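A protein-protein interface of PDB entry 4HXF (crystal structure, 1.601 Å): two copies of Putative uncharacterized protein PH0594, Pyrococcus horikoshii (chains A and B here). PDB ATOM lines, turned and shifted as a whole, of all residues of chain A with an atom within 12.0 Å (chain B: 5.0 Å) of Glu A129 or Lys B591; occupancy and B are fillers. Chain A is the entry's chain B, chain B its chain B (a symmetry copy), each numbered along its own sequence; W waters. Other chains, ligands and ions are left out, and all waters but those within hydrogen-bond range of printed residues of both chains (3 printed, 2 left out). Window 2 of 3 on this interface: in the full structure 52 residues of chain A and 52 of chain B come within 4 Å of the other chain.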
ATOM      1  N   ARG A 125      21.060 -18.200 -19.783  1.00  0.00           N
ATOM      2  CA  ARG A 125      20.352 -17.860 -18.542  1.00  0.00           C
ATOM      3  C   ARG A 125      21.330 -17.952 -17.385  1.00  0.00           C
ATOM      4  O   ARG A 125      22.453 -18.430 -17.587  1.00  0.00           O
ATOM      5  CB  ARG A 125      19.222 -18.868 -18.348  1.00  0.00           C
ATOM      6  CG  ARG A 125      18.183 -18.844 -19.391  1.00  0.00           C
ATOM      7  CD  ARG A 125      17.036 -19.801 -19.107  1.00  0.00           C
ATOM      8  NE  ARG A 125      16.002 -19.671 -20.118  1.00  0.00           N
ATOM      9  CZ  ARG A 125      14.989 -20.536 -20.302  1.00  0.00           C
ATOM     10  NH1 ARG A 125      14.890 -21.634 -19.474  1.00  0.00           N
ATOM     11  NH2 ARG A 125      14.110 -20.345 -21.273  1.00  0.00           N
ATOM     12  N   ARG A 126      20.912 -17.523 -16.194  1.00  0.00           N
ATOM     13  CA  ARG A 126      21.770 -17.477 -14.984  1.00  0.00           C
ATOM     14  C   ARG A 126      22.113 -18.891 -14.540  1.00  0.00           C
ATOM     15  O   ARG A 126      23.254 -19.179 -14.187  1.00  0.00           O
ATOM     16  CB  ARG A 126      21.086 -16.646 -13.892  1.00  0.00           C
ATOM     17  CG  ARG A 126      21.158 -15.141 -14.023  1.00  0.00           C
ATOM     18  CD  ARG A 126      20.172 -14.337 -13.140  1.00  0.00           C
ATOM     19  NE  ARG A 126      20.498 -12.919 -13.330  1.00  0.00           N
ATOM     20  CZ  ARG A 126      19.623 -11.944 -13.591  1.00  0.00           C
ATOM     21  NH1 ARG A 126      20.056 -10.663 -13.743  1.00  0.00           N
ATOM     22  NH2 ARG A 126      18.321 -12.220 -13.694  1.00  0.00           N
ATOM     23  N   GLU A 127      21.189 -19.822 -14.516  1.00  0.00           N
ATOM     24  CA  GLU A 127      21.460 -21.291 -14.239  1.00  0.00           C
ATOM     25  C   GLU A 127      21.899 -21.767 -12.808  1.00  0.00           C
ATOM     26  O   GLU A 127      22.494 -22.816 -12.690  1.00  0.00           O
ATOM     27  CB  GLU A 127      22.501 -21.894 -15.192  1.00  0.00           C
ATOM     28  CG  GLU A 127      22.259 -21.521 -16.657  1.00  0.00           C
ATOM     29  CD  GLU A 127      21.049 -22.141 -17.247  1.00  0.00           C
ATOM     30  OE1 GLU A 127      20.282 -22.711 -16.474  1.00  0.00           O
ATOM     31  OE2 GLU A 127      20.843 -22.079 -18.493  1.00  0.00           O
ATOM     32  N   ASP A 128      21.591 -20.981 -11.845  1.00  0.00           N
ATOM     33  CA  ASP A 128      21.863 -21.416 -10.459  1.00  0.00           C
ATOM     34  C   ASP A 128      20.991 -22.697 -10.231  1.00  0.00           C
ATOM     35  O   ASP A 128      19.770 -22.705 -10.558  1.00  0.00           O
ATOM     36  CB  ASP A 128      21.562 -20.389  -9.430  1.00  0.00           C
ATOM     37  CG  ASP A 128      21.900 -20.900  -8.035  1.00  0.00           C
ATOM     38  OD1 ASP A 128      23.110 -20.766  -7.683  1.00  0.00           O
ATOM     39  OD2 ASP A 128      21.024 -21.492  -7.290  1.00  0.00           O
ATOM     40  N   GLU A 129      21.590 -23.751  -9.603  1.00  0.00           N
ATOM     41  CA  GLU A 129      20.971 -24.985  -9.290  1.00  0.00           C
ATOM     42  C   GLU A 129      19.755 -24.885  -8.374  1.00  0.00           C
ATOM     43  O   GLU A 129      18.821 -25.697  -8.468  1.00  0.00           O
ATOM     44  CB  GLU A 129      21.975 -25.944  -8.591  1.00  0.00           C
ATOM     45  CG  GLU A 129      23.248 -25.298  -8.037  1.00  0.00           C
ATOM     46  CD  GLU A 129      24.204 -24.801  -9.127  1.00  0.00           C
ATOM     47  OE1 GLU A 129      24.705 -25.612  -9.941  1.00  0.00           O
ATOM     48  OE2 GLU A 129      24.481 -23.604  -9.183  1.00  0.00           O
ATOM     49  N   ASP A 130      19.768 -23.900  -7.508  1.00  0.00           N
ATOM     50  CA  ASP A 130      18.778 -23.813  -6.383  1.00  0.00           C
ATOM     51  C   ASP A 130      17.704 -22.753  -6.551  1.00  0.00           C
ATOM     52  O   ASP A 130      16.585 -22.896  -6.021  1.00  0.00           O
ATOM     53  CB  ASP A 130      19.470 -23.555  -5.071  1.00  0.00           C
ATOM     54  CG  ASP A 130      20.409 -24.731  -4.717  1.00  0.00           C
ATOM     55  OD1 ASP A 130      19.925 -25.874  -4.727  1.00  0.00           O
ATOM     56  OD2 ASP A 130      21.626 -24.480  -4.636  1.00  0.00           O
ATOM     57  N   PHE A 131      17.998 -21.677  -7.302  1.00  0.00           N
ATOM     58  CA  PHE A 131      17.015 -20.575  -7.460  1.00  0.00           C
ATOM     59  C   PHE A 131      17.163 -19.839  -8.805  1.00  0.00           C
ATOM     60  O   PHE A 131      18.245 -19.777  -9.407  1.00  0.00           O
ATOM     61  CB  PHE A 131      17.004 -19.565  -6.313  1.00  0.00           C
ATOM     62  CG  PHE A 131      18.214 -18.623  -6.246  1.00  0.00           C
ATOM     63  CD1 PHE A 131      19.413 -19.060  -5.745  1.00  0.00           C
ATOM     64  CD2 PHE A 131      18.127 -17.319  -6.746  1.00  0.00           C
ATOM     65  CE1 PHE A 131      20.515 -18.242  -5.697  1.00  0.00           C
ATOM     66  CE2 PHE A 131      19.232 -16.449  -6.690  1.00  0.00           C
ATOM     67  CZ  PHE A 131      20.430 -16.916  -6.133  1.00  0.00           C
ATOM     68  N   ILE A 132      16.025 -19.428  -9.304  1.00  0.00           N
ATOM     69  CA  ILE A 132      15.813 -18.531 -10.437  1.00  0.00           C
ATOM     70  C   ILE A 132      15.855 -17.132  -9.909  1.00  0.00           C
ATOM     71  O   ILE A 132      15.323 -16.841  -8.805  1.00  0.00           O
ATOM     72  CB  ILE A 132      14.412 -18.842 -11.002  1.00  0.00           C
ATOM     73  CG1 ILE A 132      14.411 -20.281 -11.591  1.00  0.00           C
ATOM     74  CG2 ILE A 132      13.965 -17.816 -12.015  1.00  0.00           C
ATOM     75  CD1 ILE A 132      13.117 -20.981 -11.324  1.00  0.00           C
ATOM     76  N   PHE A 133      16.504 -16.179 -10.572  1.00  0.00           N
ATOM     77  CA  PHE A 133      16.504 -14.821 -10.147  1.00  0.00           C
ATOM     78  C   PHE A 133      16.080 -13.921 -11.273  1.00  0.00           C
ATOM     79  O   PHE A 133      16.617 -14.108 -12.413  1.00  0.00           O
ATOM     80  CB  PHE A 133      17.883 -14.394  -9.720  1.00  0.00           C
ATOM     81  CG  PHE A 133      17.917 -13.086  -9.052  1.00  0.00           C
ATOM     82  CD1 PHE A 133      17.457 -12.950  -7.743  1.00  0.00           C
ATOM     83  CD2 PHE A 133      18.326 -11.946  -9.716  1.00  0.00           C
ATOM     84  CE1 PHE A 133      17.442 -11.698  -7.184  1.00  0.00           C
ATOM     85  CE2 PHE A 133      18.238 -10.692  -9.155  1.00  0.00           C
ATOM     86  CZ  PHE A 133      17.833 -10.573  -7.867  1.00  0.00           C
ATOM     87  N   PHE A 146      11.119 -20.743 -16.916  1.00  0.00           N
ATOM     88  CA  PHE A 146      11.514 -19.498 -16.214  1.00  0.00           C
ATOM     89  C   PHE A 146      12.642 -18.857 -17.006  1.00  0.00           C
ATOM     90  O   PHE A 146      13.631 -19.530 -17.380  1.00  0.00           O
ATOM     91  CB  PHE A 146      11.940 -19.711 -14.770  1.00  0.00           C
ATOM     92  CG  PHE A 146      10.825 -20.065 -13.866  1.00  0.00           C
ATOM     93  CD1 PHE A 146      10.429 -21.396 -13.688  1.00  0.00           C
ATOM     94  CD2 PHE A 146      10.087 -19.067 -13.246  1.00  0.00           C
ATOM     95  CE1 PHE A 146       9.403 -21.746 -12.814  1.00  0.00           C
ATOM     96  CE2 PHE A 146       9.025 -19.403 -12.411  1.00  0.00           C
ATOM     97  CZ  PHE A 146       8.711 -20.755 -12.141  1.00  0.00           C
ATOM     98  N   ASP A 148      14.957 -16.663 -15.964  1.00  0.00           N
ATOM     99  CA  ASP A 148      16.204 -16.668 -15.247  1.00  0.00           C
ATOM    100  C   ASP A 148      17.267 -15.708 -15.831  1.00  0.00           C
ATOM    101  O   ASP A 148      18.395 -16.126 -16.030  1.00  0.00           O
ATOM    102  CB  ASP A 148      16.671 -18.116 -15.156  1.00  0.00           C
ATOM    103  CG  ASP A 148      17.693 -18.356 -14.028  1.00  0.00           C
ATOM    104  OD1 ASP A 148      17.807 -17.567 -13.061  1.00  0.00           O
ATOM    105  OD2 ASP A 148      18.414 -19.312 -14.324  1.00  0.00           O
ATOM    106  N   PHE B 573      13.039 -19.999  -5.454  1.00  0.00           N
ATOM    107  CA  PHE B 573      13.745 -21.228  -5.163  1.00  0.00           C
ATOM    108  C   PHE B 573      12.967 -22.413  -5.733  1.00  0.00           C
ATOM    109  O   PHE B 573      11.742 -22.459  -5.651  1.00  0.00           O
ATOM    110  CB  PHE B 573      13.893 -21.348  -3.641  1.00  0.00           C
ATOM    111  CG  PHE B 573      15.027 -20.478  -3.070  1.00  0.00           C
ATOM    112  CD1 PHE B 573      14.828 -19.111  -2.942  1.00  0.00           C
ATOM    113  CD2 PHE B 573      16.338 -20.967  -2.875  1.00  0.00           C
ATOM    114  CE1 PHE B 573      15.828 -18.293  -2.526  1.00  0.00           C
ATOM    115  CE2 PHE B 573      17.330 -20.125  -2.477  1.00  0.00           C
ATOM    116  CZ  PHE B 573      17.105 -18.787  -2.353  1.00  0.00           C
ATOM    117  N   LYS B 574      13.691 -23.244  -6.417  1.00  0.00           N
ATOM    118  CA  LYS B 574      13.153 -24.300  -7.274  1.00  0.00           C
ATOM    119  C   LYS B 574      12.536 -25.407  -6.426  1.00  0.00           C
ATOM    120  O   LYS B 574      11.597 -26.061  -6.908  1.00  0.00           O
ATOM    121  CB  LYS B 574      14.245 -24.866  -8.162  1.00  0.00           C
ATOM    122  CG  LYS B 574      14.802 -23.854  -9.205  1.00  0.00           C
ATOM    123  CD  LYS B 574      15.571 -24.683 -10.217  1.00  0.00           C
ATOM    124  CE  LYS B 574      16.510 -23.785 -10.991  1.00  0.00           C
ATOM    125  NZ  LYS B 574      17.501 -24.530 -11.779  1.00  0.00           N
ATOM    126  N   ARG B 587      22.400 -26.210   1.043  1.00  0.00           N
ATOM    127  CA  ARG B 587      22.927 -25.266   0.035  1.00  0.00           C
ATOM    128  C   ARG B 587      21.912 -24.221  -0.386  1.00  0.00           C
ATOM    129  O   ARG B 587      22.205 -22.997  -0.565  1.00  0.00           O
ATOM    130  CB  ARG B 587      23.427 -26.052  -1.216  1.00  0.00           C
ATOM    131  CG  ARG B 587      24.198 -25.237  -2.261  1.00  0.00           C
ATOM    132  CD  ARG B 587      24.560 -26.084  -3.499  1.00  0.00           C
ATOM    133  NE  ARG B 587      23.332 -26.525  -4.179  1.00  0.00           N
ATOM    134  CZ  ARG B 587      23.033 -27.763  -4.577  1.00  0.00           C
ATOM    135  NH1 ARG B 587      23.882 -28.804  -4.430  1.00  0.00           N
ATOM    136  NH2 ARG B 587      21.855 -28.019  -5.116  1.00  0.00           N
ATOM    137  N   HIS B 588      20.678 -24.651  -0.554  1.00  0.00           N
ATOM    138  CA  HIS B 588      19.554 -23.733  -0.739  1.00  0.00           C
ATOM    139  C   HIS B 588      19.461 -22.659   0.367  1.00  0.00           C
ATOM    140  O   HIS B 588      19.386 -21.456   0.134  1.00  0.00           O
ATOM    141  CB  HIS B 588      18.291 -24.610  -0.816  1.00  0.00           C
ATOM    142  CG  HIS B 588      16.965 -23.896  -0.661  1.00  0.00           C
ATOM    143  ND1 HIS B 588      15.871 -24.237  -1.436  1.00  0.00           N
ATOM    144  CD2 HIS B 588      16.524 -22.936   0.207  1.00  0.00           C
ATOM    145  CE1 HIS B 588      14.796 -23.573  -0.987  1.00  0.00           C
ATOM    146  NE2 HIS B 588      15.162 -22.748  -0.021  1.00  0.00           N
ATOM    147  N   ARG B 589      19.536 -23.112   1.635  1.00  0.00           N
ATOM    148  CA  ARG B 589      19.438 -22.188   2.714  1.00  0.00           C
ATOM    149  C   ARG B 589      20.595 -21.232   2.815  1.00  0.00           C
ATOM    150  O   ARG B 589      20.400 -20.067   3.096  1.00  0.00           O
ATOM    151  CB  ARG B 589      19.344 -23.012   4.016  1.00  0.00           C
ATOM    152  CG  ARG B 589      17.970 -23.641   4.216  1.00  0.00           C
ATOM    153  CD  ARG B 589      17.972 -24.519   5.454  1.00  0.00           C
ATOM    154  NE  ARG B 589      18.022 -23.650   6.572  1.00  0.00           N
ATOM    155  CZ  ARG B 589      18.453 -24.008   7.810  1.00  0.00           C
ATOM    156  NH1 ARG B 589      18.763 -25.267   8.048  1.00  0.00           N
ATOM    157  NH2 ARG B 589      18.521 -23.095   8.811  1.00  0.00           N
ATOM    158  N   MET B 590      21.799 -21.707   2.553  1.00  0.00           N
ATOM    159  CA  MET B 590      23.012 -20.862   2.510  1.00  0.00           C
ATOM    160  C   MET B 590      22.837 -19.705   1.491  1.00  0.00           C
ATOM    161  O   MET B 590      23.142 -18.543   1.767  1.00  0.00           O
ATOM    162  CB  MET B 590      24.159 -21.749   2.177  1.00  0.00           C
ATOM    163  CG  MET B 590      25.464 -21.025   2.101  1.00  0.00           C
ATOM    164  SD  MET B 590      25.828 -20.370   0.483  1.00  0.00           S
ATOM    165  CE  MET B 590      25.710 -21.829  -0.576  1.00  0.00           C
ATOM    166  N   LYS B 591      22.300 -20.062   0.312  1.00  0.00           N
ATOM    167  CA  LYS B 591      22.132 -19.085  -0.803  1.00  0.00           C
ATOM    168  C   LYS B 591      21.055 -18.100  -0.419  1.00  0.00           C
ATOM    169  O   LYS B 591      21.244 -16.872  -0.640  1.00  0.00           O
ATOM    170  CB  LYS B 591      21.770 -19.726  -2.138  1.00  0.00           C
ATOM    171  CG  LYS B 591      22.980 -20.516  -2.726  1.00  0.00           C
ATOM    172  CD  LYS B 591      22.591 -21.246  -3.998  1.00  0.00           C
ATOM    173  CE  LYS B 591      23.843 -21.891  -4.529  1.00  0.00           C
ATOM    174  NZ  LYS B 591      23.571 -22.755  -5.706  1.00  0.00           N
ATOM    175  N   ARG B 592      19.992 -18.537   0.243  1.00  0.00           N
ATOM    176  CA  ARG B 592      19.002 -17.588   0.740  1.00  0.00           C
ATOM    177  C   ARG B 592      19.588 -16.648   1.754  1.00  0.00           C
ATOM    178  O   ARG B 592      19.348 -15.427   1.688  1.00  0.00           O
ATOM    179  CB  ARG B 592      17.763 -18.298   1.332  1.00  0.00           C
ATOM    180  CG  ARG B 592      16.795 -17.316   1.947  1.00  0.00           C
ATOM    181  CD  ARG B 592      15.605 -17.932   2.596  1.00  0.00           C
ATOM    182  NE  ARG B 592      14.992 -16.968   3.539  1.00  0.00           N
ATOM    183  CZ  ARG B 592      15.438 -16.675   4.756  1.00  0.00           C
ATOM    184  NH1 ARG B 592      14.837 -15.736   5.478  1.00  0.00           N
ATOM    185  NH2 ARG B 592      16.442 -17.338   5.308  1.00  0.00           N
ATOM    186  N   TYR B 593      20.337 -17.178   2.734  1.00  0.00           N
ATOM    187  CA  TYR B 593      20.935 -16.289   3.722  1.00  0.00           C
ATOM    188  C   TYR B 593      21.869 -15.262   3.092  1.00  0.00           C
ATOM    189  O   TYR B 593      21.897 -14.084   3.509  1.00  0.00           O
ATOM    190  CB  TYR B 593      21.648 -17.058   4.836  1.00  0.00           C
ATOM    191  CG  TYR B 593      20.778 -17.916   5.764  1.00  0.00           C
ATOM    192  CD1 TYR B 593      21.079 -19.278   5.979  1.00  0.00           C
ATOM    193  CD2 TYR B 593      19.732 -17.376   6.411  1.00  0.00           C
ATOM    194  CE1 TYR B 593      20.334 -20.001   6.899  1.00  0.00           C
ATOM    195  CE2 TYR B 593      18.911 -18.109   7.275  1.00  0.00           C
ATOM    196  CZ  TYR B 593      19.255 -19.446   7.512  1.00  0.00           C
ATOM    197  OH  TYR B 593      18.495 -20.190   8.394  1.00  0.00           O
ATOM    198  N   LYS B 594      22.623 -15.659   2.057  1.00  0.00           N
ATOM    199  CA  LYS B 594      23.591 -14.757   1.480  1.00  0.00           C
ATOM    200  C   LYS B 594      22.833 -13.670   0.675  1.00  0.00           C
ATOM    201  O   LYS B 594      23.135 -12.446   0.729  1.00  0.00           O
ATOM    202  CB  LYS B 594      24.500 -15.551   0.560  1.00  0.00           C
ATOM    203  CG  LYS B 594      25.502 -14.661  -0.155  1.00  0.00           C
ATOM    204  CD  LYS B 594      26.422 -13.880   0.781  1.00  0.00           C
ATOM    205  CE  LYS B 594      27.630 -13.266   0.060  1.00  0.00           C
ATOM    206  NZ  LYS B 594      28.495 -12.361   0.893  1.00  0.00           N
ATOM    207  N   LEU B 595      21.738 -14.065  -0.029  1.00  0.00           N
ATOM    208  CA  LEU B 595      20.858 -13.083  -0.726  1.00  0.00           C
ATOM    209  C   LEU B 595      20.264 -12.062   0.247  1.00  0.00           C
ATOM    210  O   LEU B 595      20.257 -10.855   0.003  1.00  0.00           O
ATOM    211  CB  LEU B 595      19.697 -13.741  -1.489  1.00  0.00           C
ATOM    212  CG  LEU B 595      19.969 -14.543  -2.756  1.00  0.00           C
ATOM    213  CD1 LEU B 595      18.718 -15.308  -3.198  1.00  0.00           C
ATOM    214  CD2 LEU B 595      20.446 -13.547  -3.836  1.00  0.00           C
ATOM    215  N   PHE B 596      19.759 -12.581   1.368  1.00  0.00           N
ATOM    216  CA  PHE B 596      19.111 -11.772   2.353  1.00  0.00           C
ATOM    217  C   PHE B 596      20.105 -10.745   2.874  1.00  0.00           C
ATOM    218  O   PHE B 596      19.825  -9.531   2.928  1.00  0.00           O
ATOM    219  CB  PHE B 596      18.639 -12.699   3.463  1.00  0.00           C
ATOM    220  CG  PHE B 596      17.890 -12.044   4.630  1.00  0.00           C
ATOM    221  CD1 PHE B 596      16.507 -12.085   4.694  1.00  0.00           C
ATOM    222  CD2 PHE B 596      18.583 -11.492   5.712  1.00  0.00           C
ATOM    223  CE1 PHE B 596      15.823 -11.502   5.740  1.00  0.00           C
ATOM    224  CE2 PHE B 596      17.912 -10.977   6.803  1.00  0.00           C
ATOM    225  CZ  PHE B 596      16.516 -10.930   6.782  1.00  0.00           C
ATOM    226  N   LEU B 617      26.880 -13.138  -5.395  1.00  0.00           N
ATOM    227  CA  LEU B 617      26.904 -14.494  -4.802  1.00  0.00           C
ATOM    228  C   LEU B 617      28.145 -15.340  -5.101  1.00  0.00           C
ATOM    229  O   LEU B 617      28.396 -16.299  -4.377  1.00  0.00           O
ATOM    230  CB  LEU B 617      25.606 -15.291  -5.106  1.00  0.00           C
ATOM    231  CG  LEU B 617      24.572 -15.303  -3.963  1.00  0.00           C
ATOM    232  CD1 LEU B 617      23.887 -13.933  -3.788  1.00  0.00           C
ATOM    233  CD2 LEU B 617      23.565 -16.450  -4.152  1.00  0.00           C
HETATM  234  O   HOH W   1      15.773 -24.810  -4.175  1.00  0.00           O
HETATM  235  O   HOH W   2      25.867 -24.169  -6.185  1.00  0.00           O
HETATM  236  O   HOH W   3      18.149 -27.031 -11.099  1.00  0.00           O
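Of the 11 printed residues of chain A, 5 touch a printed residue of chain B. Hydrophobic or aromatic side chains of chain A that line the printed part of chain B: Phe A131 and Ile A132. Printed residues of chain B that touch a printed residue of chain A: Phe B573, Lys B574, Arg B587, Lys B591, Leu B595 and Leu B617. Hydrophobic or aromatic side chains of chain B that line the printed part of chain A: Phe B573, Leu B595 and Leu B617. Among the printed residues, Asp or Glu carboxylates within 4 Å of a Lys or Arg side-chain nitrogen of the other chain: Asp A128 with Lys B591 (2.8 Å), Glu A129 with Lys B591 (3.7 Å), Asp A130 with Arg B587 (2.7 Å) and Asp A130 with Lys B591 (2.8 Å).
The backbone NH (N) of Asp A130 is in hydrogen-bond range of the side-chain carboxylate (OD2) of Asp A128. OD2 of Asp A128 sits at hydrogen-bond distance from N of Phe A131 (3.0 Å).
The side-chain amino group of Lys B574 sits at hydrogen-bond distance from the backbone carbonyl oxygen of Asp A128, 3.2 Å away. The side-chain carboxylate of Asp A128 is in salt-bridge range of the side-chain amino group of Lys B591, at 2.8 Å. OE2 of Glu A129 lies within salt-bridge range of NZ of Lys B591, 3.7 Å away. The backbone carbonyl oxygen of Asp A130 is in hydrogen-bond range of the backbone NH of Lys B574, at 2.9 Å. The side-chain carboxylate of Asp A130 lies within salt-bridge range of the guanidinium group of Arg B587 (2.7 Å). The side-chain amino group (NZ) of Lys B591 is in salt-bridge range of the side-chain carboxylate (OD2) of Asp A130 (2.8 Å).
Arg A125 touches none of the printed residues of chain B. Of the printed residues of chain B, Asp A128 touches Lys B574 and Lys B591. Of the printed residues of chain B, Glu A129 touches Lys B574 (3.8 Å) and Lys B591 (3.5 Å). Printed residues of chain B within 4 Å of Ile A132: Lys B574 (3.9 Å). Printed residues of chain A within 4 Å of Phe B573: Asp A130 (3.4 Å) and Phe A131 (3.8 Å). Printed residues of chain A within 4 Å of Lys B574: Asp A128, Glu A129, Asp A130 and Ile A132. Of the printed residues of chain A, Lys B591 touches Asp A128 (2.8 Å), Glu A129 (3.5 Å) and Asp A130 (2.8 Å). Of the printed residues of chain A, Leu B595 touches Phe A131. The nearest printed residue of chain B that does not touch Glu A129 is Arg B587 (4.05 Å).
Water W3 bridges the side-chain amino group of Lys B574 (2.7 Å) and the backbone carbonyl oxygen of Glu A129 (3.0 Å). Water W2 lies within hydrogen-bond range of NZ of Lys B591 and OE2 of Glu A129. Water W1 lies within hydrogen-bond range of O of Asp A130 (2.8 Å), ND1 of His B588 (2.8 Å) and N of Lys B574 (3.4 Å).
No position is printed for both chains.
O of Glu A129 touches NZ of Lys B574 (3.8 Å). Phe B573 touches Asp A130 (CA to O, 3.4 Å). Phe B573 touches Phe A131. Phe A131 touches Leu B595. Phe A131 touches Leu B617. CD1 of Ile A132 touches CG of Lys B574 (3.9 Å).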
